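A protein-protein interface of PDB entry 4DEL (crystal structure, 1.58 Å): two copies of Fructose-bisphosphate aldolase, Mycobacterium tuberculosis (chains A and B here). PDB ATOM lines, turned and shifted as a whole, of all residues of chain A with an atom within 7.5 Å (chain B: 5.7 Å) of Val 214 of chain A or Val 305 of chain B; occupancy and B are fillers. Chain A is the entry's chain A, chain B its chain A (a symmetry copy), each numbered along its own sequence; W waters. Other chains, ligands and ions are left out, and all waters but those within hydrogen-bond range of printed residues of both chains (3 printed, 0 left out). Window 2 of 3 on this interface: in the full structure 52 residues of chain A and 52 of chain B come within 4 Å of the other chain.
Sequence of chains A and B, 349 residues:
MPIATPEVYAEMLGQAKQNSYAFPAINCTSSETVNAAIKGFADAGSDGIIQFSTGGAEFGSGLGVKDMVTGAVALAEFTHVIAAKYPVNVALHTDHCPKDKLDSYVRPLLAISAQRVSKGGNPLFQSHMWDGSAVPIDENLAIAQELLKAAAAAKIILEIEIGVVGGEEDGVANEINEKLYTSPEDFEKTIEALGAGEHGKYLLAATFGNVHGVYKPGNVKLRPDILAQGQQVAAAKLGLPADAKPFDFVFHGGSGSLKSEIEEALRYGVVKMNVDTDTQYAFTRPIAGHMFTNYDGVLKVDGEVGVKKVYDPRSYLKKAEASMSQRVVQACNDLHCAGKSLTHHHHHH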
ATOM      1  N   VAL A 211      12.059 -18.431   4.289  1.00  0.00           N
ATOM      2  CA  VAL A 211      11.660 -18.946   2.983  1.00  0.00           C
ATOM      3  C   VAL A 211      10.900 -20.270   3.171  1.00  0.00           C
ATOM      4  O   VAL A 211      11.400 -21.167   3.855  1.00  0.00           O
ATOM      5  CB  VAL A 211      12.897 -19.160   2.053  1.00  0.00           C
ATOM      6  CG1 VAL A 211      12.476 -19.769   0.731  1.00  0.00           C
ATOM      7  CG2 VAL A 211      13.627 -17.833   1.799  1.00  0.00           C
ATOM      8  N   HIS A 212       9.714 -20.362   2.582  1.00  0.00           N
ATOM      9  CA  HIS A 212       8.929 -21.601   2.581  1.00  0.00           C
ATOM     10  C   HIS A 212       9.658 -22.612   1.706  1.00  0.00           C
ATOM     11  O   HIS A 212      10.098 -22.274   0.598  1.00  0.00           O
ATOM     12  CB  HIS A 212       7.547 -21.339   1.995  1.00  0.00           C
ATOM     13  CG  HIS A 212       6.609 -20.626   2.922  1.00  0.00           C
ATOM     14  ND1 HIS A 212       5.841 -19.554   2.515  1.00  0.00           N
ATOM     15  CD2 HIS A 212       6.313 -20.829   4.228  1.00  0.00           C
ATOM     16  CE1 HIS A 212       5.089 -19.146   3.526  1.00  0.00           C
ATOM     17  NE2 HIS A 212       5.363 -19.899   4.575  1.00  0.00           N
ATOM     18  N   GLY A 213       9.766 -23.845   2.188  1.00  0.00           N
ATOM     19  CA  GLY A 213      10.395 -24.929   1.418  1.00  0.00           C
ATOM     20  C   GLY A 213      11.731 -25.361   1.992  1.00  0.00           C
ATOM     21  O   GLY A 213      12.128 -24.908   3.085  1.00  0.00           O
ATOM     22  N   VAL A 214      12.414 -26.253   1.268  1.00  0.00           N
ATOM     23  CA  VAL A 214      13.684 -26.819   1.705  1.00  0.00           C
ATOM     24  C   VAL A 214      14.683 -26.726   0.567  1.00  0.00           C
ATOM     25  O   VAL A 214      14.514 -27.357  -0.480  1.00  0.00           O
ATOM     26  CB  VAL A 214      13.541 -28.284   2.225  1.00  0.00           C
ATOM     27  CG1 VAL A 214      14.894 -28.955   2.444  1.00  0.00           C
ATOM     28  CG2 VAL A 214      12.728 -28.309   3.519  1.00  0.00           C
ATOM     29  N   TYR A 215      15.693 -25.897   0.792  1.00  0.00           N
ATOM     30  CA  TYR A 215      16.782 -25.657  -0.140  1.00  0.00           C
ATOM     31  C   TYR A 215      18.035 -26.281   0.470  1.00  0.00           C
ATOM     32  O   TYR A 215      18.001 -26.751   1.605  1.00  0.00           O
ATOM     33  CB  TYR A 215      16.944 -24.138  -0.327  1.00  0.00           C
ATOM     34  CG  TYR A 215      15.739 -23.480  -0.980  1.00  0.00           C
ATOM     35  CD1 TYR A 215      14.545 -23.261  -0.269  1.00  0.00           C
ATOM     36  CD2 TYR A 215      15.793 -23.066  -2.310  1.00  0.00           C
ATOM     37  CE1 TYR A 215      13.431 -22.665  -0.891  1.00  0.00           C
ATOM     38  CE2 TYR A 215      14.705 -22.453  -2.932  1.00  0.00           C
ATOM     39  CZ  TYR A 215      13.523 -22.256  -2.224  1.00  0.00           C
ATOM     40  OH  TYR A 215      12.455 -21.653  -2.867  1.00  0.00           O
ATOM     41  N   LYS A 216      19.147 -26.293  -0.260  1.00  0.00           N
ATOM     42  CA  LYS A 216      20.359 -26.889   0.296  1.00  0.00           C
ATOM     43  C   LYS A 216      20.694 -26.212   1.637  1.00  0.00           C
ATOM     44  O   LYS A 216      20.557 -24.988   1.746  1.00  0.00           O
ATOM     45  CB  LYS A 216      21.511 -26.830  -0.715  1.00  0.00           C
ATOM     46  CG  LYS A 216      21.246 -27.742  -1.916  1.00  0.00           C
ATOM     47  CD  LYS A 216      22.437 -27.904  -2.830  1.00  0.00           C
ATOM     48  CE  LYS A 216      22.151 -28.974  -3.877  1.00  0.00           C
ATOM     49  NZ  LYS A 216      23.225 -29.037  -4.910  1.00  0.00           N
ATOM     50  N   PRO A 217      21.060 -27.002   2.675  1.00  0.00           N
ATOM     51  CA  PRO A 217      21.338 -26.407   3.989  1.00  0.00           C
ATOM     52  C   PRO A 217      22.275 -25.209   3.902  1.00  0.00           C
ATOM     53  O   PRO A 217      23.352 -25.301   3.303  1.00  0.00           O
ATOM     54  CB  PRO A 217      21.992 -27.556   4.764  1.00  0.00           C
ATOM     55  CG  PRO A 217      21.384 -28.775   4.173  1.00  0.00           C
ATOM     56  CD  PRO A 217      21.227 -28.468   2.704  1.00  0.00           C
ATOM     57  N   VAL A 220      19.405 -20.533   2.580  1.00  0.00           N
ATOM     58  CA  VAL A 220      18.465 -19.555   3.121  1.00  0.00           C
ATOM     59  C   VAL A 220      19.151 -18.808   4.263  1.00  0.00           C
ATOM     60  O   VAL A 220      19.550 -19.424   5.250  1.00  0.00           O
ATOM     61  CB  VAL A 220      17.186 -20.254   3.625  1.00  0.00           C
ATOM     62  CG1 VAL A 220      16.269 -19.275   4.378  1.00  0.00           C
ATOM     63  CG2 VAL A 220      16.466 -20.914   2.451  1.00  0.00           C
ATOM     64  N   GLY A 253       8.512 -20.890   7.529  1.00  0.00           N
ATOM     65  CA  GLY A 253       9.540 -21.552   6.742  1.00  0.00           C
ATOM     66  C   GLY A 253      10.500 -22.366   7.583  1.00  0.00           C
ATOM     67  O   GLY A 253      11.681 -22.474   7.245  1.00  0.00           O
ATOM     68  N   GLY A 254       9.996 -22.970   8.661  1.00  0.00           N
ATOM     69  CA  GLY A 254      10.827 -23.740   9.598  1.00  0.00           C
ATOM     70  C   GLY A 254      11.636 -24.893   9.009  1.00  0.00           C
ATOM     71  O   GLY A 254      12.784 -25.121   9.387  1.00  0.00           O
ATOM     72  N   SER A 255      11.056 -25.599   8.046  1.00  0.00           N
ATOM     73  CA  SER A 255      11.743 -26.759   7.456  1.00  0.00           C
ATOM     74  C   SER A 255      13.077 -26.355   6.859  1.00  0.00           C
ATOM     75  O   SER A 255      13.172 -25.311   6.223  1.00  0.00           O
ATOM     76  CB  SER A 255      10.894 -27.364   6.343  1.00  0.00           C
ATOM     77  OG  SER A 255       9.647 -27.836   6.838  1.00  0.00           O
ATOM     78  N   GLY A 256      14.089 -27.200   7.031  1.00  0.00           N
ATOM     79  CA  GLY A 256      15.392 -26.979   6.399  1.00  0.00           C
ATOM     80  C   GLY A 256      16.282 -25.974   7.117  1.00  0.00           C
ATOM     81  O   GLY A 256      17.425 -25.736   6.697  1.00  0.00           O
ATOM     82  N   SER A 257      15.767 -25.388   8.194  1.00  0.00           N
ATOM     83  CA  SER A 257      16.538 -24.417   8.977  1.00  0.00           C
ATOM     84  C   SER A 257      17.681 -25.080   9.735  1.00  0.00           C
ATOM     85  O   SER A 257      17.596 -26.250  10.151  1.00  0.00           O
ATOM     86  CB  SER A 257      15.631 -23.683   9.971  1.00  0.00           C
ATOM     87  OG  SER A 257      14.641 -22.943   9.293  1.00  0.00           O
ATOM     88  N   ASP A 276       6.142 -27.594   7.450  1.00  0.00           N
ATOM     89  CA  ASP A 276       5.282 -28.245   6.449  1.00  0.00           C
ATOM     90  C   ASP A 276       6.149 -29.096   5.530  1.00  0.00           C
ATOM     91  O   ASP A 276       6.005 -30.325   5.508  1.00  0.00           O
ATOM     92  CB  ASP A 276       4.473 -27.203   5.650  1.00  0.00           C
ATOM     93  CG  ASP A 276       3.348 -27.817   4.824  1.00  0.00           C
ATOM     94  OD1 ASP A 276       3.210 -29.071   4.804  1.00  0.00           O
ATOM     95  OD2 ASP A 276       2.570 -27.031   4.216  1.00  0.00           O
ATOM     96  N   THR A 277       7.081 -28.453   4.819  1.00  0.00           N
ATOM     97  CA  THR A 277       7.875 -29.157   3.797  1.00  0.00           C
ATOM     98  C   THR A 277       8.613 -30.402   4.337  1.00  0.00           C
ATOM     99  O   THR A 277       8.600 -31.465   3.694  1.00  0.00           O
ATOM    100  CB  THR A 277       8.849 -28.202   3.089  1.00  0.00           C
ATOM    101  OG1 THR A 277       8.118 -27.093   2.550  1.00  0.00           O
ATOM    102  CG2 THR A 277       9.539 -28.913   1.925  1.00  0.00           C
ATOM    103  N   ASP A 278       9.237 -30.287   5.515  1.00  0.00           N
ATOM    104  CA  ASP A 278       9.980 -31.413   6.094  1.00  0.00           C
ATOM    105  C   ASP A 278       9.083 -32.565   6.514  1.00  0.00           C
ATOM    106  O   ASP A 278       9.449 -33.714   6.351  1.00  0.00           O
ATOM    107  CB  ASP A 278      10.845 -30.971   7.273  1.00  0.00           C
ATOM    108  CG  ASP A 278      12.242 -30.510   6.839  1.00  0.00           C
ATOM    109  OD1 ASP A 278      12.640 -30.739   5.676  1.00  0.00           O
ATOM    110  OD2 ASP A 278      12.944 -29.918   7.690  1.00  0.00           O
ATOM    111  N   THR A 279       7.903 -32.257   7.046  1.00  0.00           N
ATOM    112  CA  THR A 279       6.952 -33.314   7.386  1.00  0.00           C
ATOM    113  C   THR A 279       6.323 -33.931   6.124  1.00  0.00           C
ATOM    114  O   THR A 279       5.965 -35.104   6.132  1.00  0.00           O
ATOM    115  CB  THR A 279       5.881 -32.852   8.419  1.00  0.00           C
ATOM    116  OG1 THR A 279       5.504 -31.493   8.164  1.00  0.00           O
ATOM    117  CG2 THR A 279       6.456 -32.962   9.824  1.00  0.00           C
ATOM    118  N   TYR A 281       8.075 -34.376   3.300  1.00  0.00           N
ATOM    119  CA  TYR A 281       9.102 -35.349   2.897  1.00  0.00           C
ATOM    120  C   TYR A 281       9.088 -36.611   3.781  1.00  0.00           C
ATOM    121  O   TYR A 281       9.194 -37.750   3.288  1.00  0.00           O
ATOM    122  CB  TYR A 281      10.509 -34.729   2.895  1.00  0.00           C
ATOM    123  CG  TYR A 281      11.551 -35.688   2.318  1.00  0.00           C
ATOM    124  CD1 TYR A 281      11.629 -35.906   0.938  1.00  0.00           C
ATOM    125  CD2 TYR A 281      12.433 -36.383   3.152  1.00  0.00           C
ATOM    126  CE1 TYR A 281      12.570 -36.814   0.406  1.00  0.00           C
ATOM    127  CE2 TYR A 281      13.378 -37.287   2.630  1.00  0.00           C
ATOM    128  CZ  TYR A 281      13.434 -37.497   1.263  1.00  0.00           C
ATOM    129  OH  TYR A 281      14.363 -38.376   0.740  1.00  0.00           O
ATOM    130  N   ARG A 327       9.423 -37.131  12.578  1.00  0.00           N
ATOM    131  CA  ARG A 327       9.875 -35.790  12.235  1.00  0.00           C
ATOM    132  C   ARG A 327       9.247 -34.747  13.155  1.00  0.00           C
ATOM    133  O   ARG A 327       9.874 -33.733  13.463  1.00  0.00           O
ATOM    134  CB  ARG A 327       9.604 -35.467  10.759  1.00  0.00           C
ATOM    135  CG  ARG A 327      10.145 -34.081  10.291  1.00  0.00           C
ATOM    136  CD  ARG A 327      11.660 -33.942  10.525  1.00  0.00           C
ATOM    137  NE  ARG A 327      12.166 -32.634  10.099  1.00  0.00           N
ATOM    138  CZ  ARG A 327      12.136 -31.529  10.856  1.00  0.00           C
ATOM    139  NH1 ARG A 327      11.596 -31.537  12.080  1.00  0.00           N
ATOM    140  NH2 ARG A 327      12.627 -30.391  10.375  1.00  0.00           N
ATOM    141  N   GLY B 297      12.547 -36.829  -7.491  1.00  0.00           N
ATOM    142  CA  GLY B 297      11.890 -35.718  -6.793  1.00  0.00           C
ATOM    143  C   GLY B 297      11.370 -36.167  -5.441  1.00  0.00           C
ATOM    144  O   GLY B 297      11.464 -35.425  -4.449  1.00  0.00           O
ATOM    145  N   LEU B 299      12.678 -38.732  -3.774  1.00  0.00           N
ATOM    146  CA  LEU B 299      13.879 -39.127  -3.031  1.00  0.00           C
ATOM    147  C   LEU B 299      14.931 -38.037  -3.164  1.00  0.00           C
ATOM    148  O   LEU B 299      15.035 -37.397  -4.216  1.00  0.00           O
ATOM    149  CB  LEU B 299      14.470 -40.420  -3.586  1.00  0.00           C
ATOM    150  CG  LEU B 299      13.548 -41.642  -3.637  1.00  0.00           C
ATOM    151  CD1 LEU B 299      14.273 -42.729  -4.403  1.00  0.00           C
ATOM    152  CD2 LEU B 299      13.198 -42.083  -2.226  1.00  0.00           C
ATOM    153  N   LYS B 300      15.686 -37.827  -2.085  1.00  0.00           N
ATOM    154  CA  LYS B 300      16.819 -36.898  -2.092  1.00  0.00           C
ATOM    155  C   LYS B 300      18.006 -37.719  -2.587  1.00  0.00           C
ATOM    156  O   LYS B 300      18.538 -38.556  -1.851  1.00  0.00           O
ATOM    157  CB  LYS B 300      17.034 -36.357  -0.669  1.00  0.00           C
ATOM    158  CG  LYS B 300      15.900 -35.397  -0.263  1.00  0.00           C
ATOM    159  CD  LYS B 300      16.051 -34.857   1.174  1.00  0.00           C
ATOM    160  CE  LYS B 300      14.890 -33.906   1.468  1.00  0.00           C
ATOM    161  NZ  LYS B 300      14.984 -33.289   2.855  1.00  0.00           N
ATOM    162  N   VAL B 301      18.357 -37.518  -3.857  1.00  0.00           N
ATOM    163  CA  VAL B 301      19.367 -38.363  -4.513  1.00  0.00           C
ATOM    164  C   VAL B 301      20.621 -37.584  -4.922  1.00  0.00           C
ATOM    165  O   VAL B 301      20.543 -36.426  -5.328  1.00  0.00           O
ATOM    166  CB  VAL B 301      18.761 -39.106  -5.740  1.00  0.00           C
ATOM    167  CG1 VAL B 301      18.361 -38.133  -6.838  1.00  0.00           C
ATOM    168  CG2 VAL B 301      19.717 -40.171  -6.277  1.00  0.00           C
ATOM    169  N   GLY B 303      22.906 -36.124  -3.452  1.00  0.00           N
ATOM    170  CA  GLY B 303      23.188 -34.881  -2.725  1.00  0.00           C
ATOM    171  C   GLY B 303      22.200 -33.757  -2.974  1.00  0.00           C
ATOM    172  O   GLY B 303      22.360 -32.657  -2.416  1.00  0.00           O
ATOM    173  N   GLU B 304      21.187 -34.014  -3.808  1.00  0.00           N
ATOM    174  CA  GLU B 304      20.119 -33.041  -4.074  1.00  0.00           C
ATOM    175  C   GLU B 304      19.064 -33.133  -2.961  1.00  0.00           C
ATOM    176  O   GLU B 304      19.090 -34.061  -2.145  1.00  0.00           O
ATOM    177  CB  GLU B 304      19.475 -33.263  -5.448  1.00  0.00           C
ATOM    178  CG  GLU B 304      20.459 -33.194  -6.616  1.00  0.00           C
ATOM    179  CD  GLU B 304      21.121 -31.845  -6.759  1.00  0.00           C
ATOM    180  OE1 GLU B 304      20.417 -30.815  -6.771  1.00  0.00           O
ATOM    181  OE2 GLU B 304      22.364 -31.819  -6.890  1.00  0.00           O
ATOM    182  N   VAL B 305      18.144 -32.171  -2.938  1.00  0.00           N
ATOM    183  CA  VAL B 305      17.183 -32.074  -1.843  1.00  0.00           C
ATOM    184  C   VAL B 305      15.759 -32.446  -2.241  1.00  0.00           C
ATOM    185  O   VAL B 305      14.817 -32.113  -1.535  1.00  0.00           O
ATOM    186  CB  VAL B 305      17.205 -30.652  -1.171  1.00  0.00           C
ATOM    187  CG1 VAL B 305      18.565 -30.396  -0.542  1.00  0.00           C
ATOM    188  CG2 VAL B 305      16.814 -29.551  -2.161  1.00  0.00           C
ATOM    189  N   GLY B 306      15.596 -33.158  -3.356  1.00  0.00           N
ATOM    190  CA  GLY B 306      14.250 -33.528  -3.799  1.00  0.00           C
ATOM    191  C   GLY B 306      13.487 -32.356  -4.387  1.00  0.00           C
ATOM    192  O   GLY B 306      14.029 -31.258  -4.540  1.00  0.00           O
ATOM    193  N   VAL B 307      12.221 -32.598  -4.713  1.00  0.00           N
ATOM    194  CA  VAL B 307      11.364 -31.607  -5.348  1.00  0.00           C
ATOM    195  C   VAL B 307      10.025 -31.580  -4.616  1.00  0.00           C
ATOM    196  O   VAL B 307       9.213 -32.503  -4.760  1.00  0.00           O
ATOM    197  CB  VAL B 307      11.167 -31.930  -6.843  1.00  0.00           C
ATOM    198  CG1 VAL B 307      10.220 -30.935  -7.510  1.00  0.00           C
ATOM    199  CG2 VAL B 307      12.533 -31.947  -7.569  1.00  0.00           C
ATOM    200  N   TYR B 311       6.881 -34.293  -3.787  1.00  0.00           N
ATOM    201  CA  TYR B 311       6.781 -35.007  -2.508  1.00  0.00           C
ATOM    202  C   TYR B 311       5.687 -34.470  -1.564  1.00  0.00           C
ATOM    203  O   TYR B 311       5.402 -35.076  -0.526  1.00  0.00           O
ATOM    204  CB  TYR B 311       8.135 -35.245  -1.816  1.00  0.00           C
ATOM    205  CG  TYR B 311       8.913 -34.072  -1.248  1.00  0.00           C
ATOM    206  CD1 TYR B 311       8.474 -33.393  -0.107  1.00  0.00           C
ATOM    207  CD2 TYR B 311      10.175 -33.738  -1.768  1.00  0.00           C
ATOM    208  CE1 TYR B 311       9.236 -32.350   0.444  1.00  0.00           C
ATOM    209  CE2 TYR B 311      10.937 -32.711  -1.224  1.00  0.00           C
ATOM    210  CZ  TYR B 311      10.472 -32.025  -0.116  1.00  0.00           C
ATOM    211  OH  TYR B 311      11.269 -31.023   0.437  1.00  0.00           O
HETATM  212  O   HOH W   1      15.193 -31.281   5.382  1.00  0.00           O
HETATM  213  O   HOH W   2      13.315 -29.903  -1.013  1.00  0.00           O
HETATM  214  O   HOH W   3      12.529 -31.906   3.042  1.00  0.00           O
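NZ of Lys 216 of chain A is in salt-bridge range of OE2 of Glu 304 of chain B, at 3.5 Å. N of Lys 300 of chain B is in hydrogen-bond range of OH of Tyr 281 of chain A (3.2 Å).
N of Thr 277 of chain A sits at hydrogen-bond distance from OG of Ser 255 of chain A (3.3 Å).
Val 214 of chain A touches Val 305 of chain B (O to CG2, 3.6 Å). Val 214 of chain A touches Tyr 311 of chain B. Gly 303 of chain B touches Lys 216 of chain A (O to CE, 3.97 Å). CG2 of Thr 277 of chain A touches OH of Tyr 311 of chain B, at 3.1 Å. Tyr 281 of chain A touches Leu 299 of chain B. N of Tyr 281 of chain A touches CD1 of Tyr 311 of chain B, at 3.6 Å.
Of the printed residues of chain B, Val 214 of chain A touches Val 305 (3.6 Å) and Tyr 311 (3.98 Å). Of the printed residues of chain A, Val 305 of chain B touches Val 214 (3.6 Å). Printed residues of chain B within 4 Å of Lys 216 of chain A: Gly 303 (3.97 Å) and Glu 304 (3.5 Å). Of the printed residues of chain A, Gly 303 of chain B touches Lys 216. Of the printed residues of chain A, Lys 300 of chain B touches Tyr 281 (3.2 Å). The nearest printed residue of chain B that does not touch Val 214 of chain A is Lys 300 of chain B (4.4 Å). The nearest printed residue of chain A that does not touch Glu 304 of chain B is Tyr 281 of chain A (7.0 Å).
Of the 10 printed residues of chain B, 6 touch a printed residue of chain A. Hydrophobic or aromatic side chains of chain B within 4 Å of the printed part of chain A: Val 305 and Tyr 311. Of the 19 printed residues of chain A, 4 touch a printed residue of chain B. Hydrophobic or aromatic side chains of chain A that line the printed part of chain B: Val 214 and Tyr 281. Among the printed residues, Asp or Glu carboxylates within 4 Å of a Lys or Arg side-chain nitrogen of the other chain: Lys 216 of chain A with Glu 304 of chain B (3.5 Å).
No position is printed for both chains. Of the 8 pairs that touch across the chains among the printed residues, none has its exchanged pair printed and touching as well.
Water W1 bridges OD1 of Asp 278 of chain A and NZ of Lys 300 of chain B. Water W2 lies within hydrogen-bond range of the backbone carbonyl oxygen of Val 305 of chain B (2.7 Å), the side-chain hydroxyl of Tyr 311 of chain B (2.7 Å) and the backbone carbonyl oxygen of Val 214 of chain A (2.9 Å). Water W3 lies within hydrogen-bond range of the side-chain amino group of Lys 300 of chain B, the side-chain carboxylate of Asp 278 of chain A and the side-chain hydroxyl of Tyr 311 of chain B.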
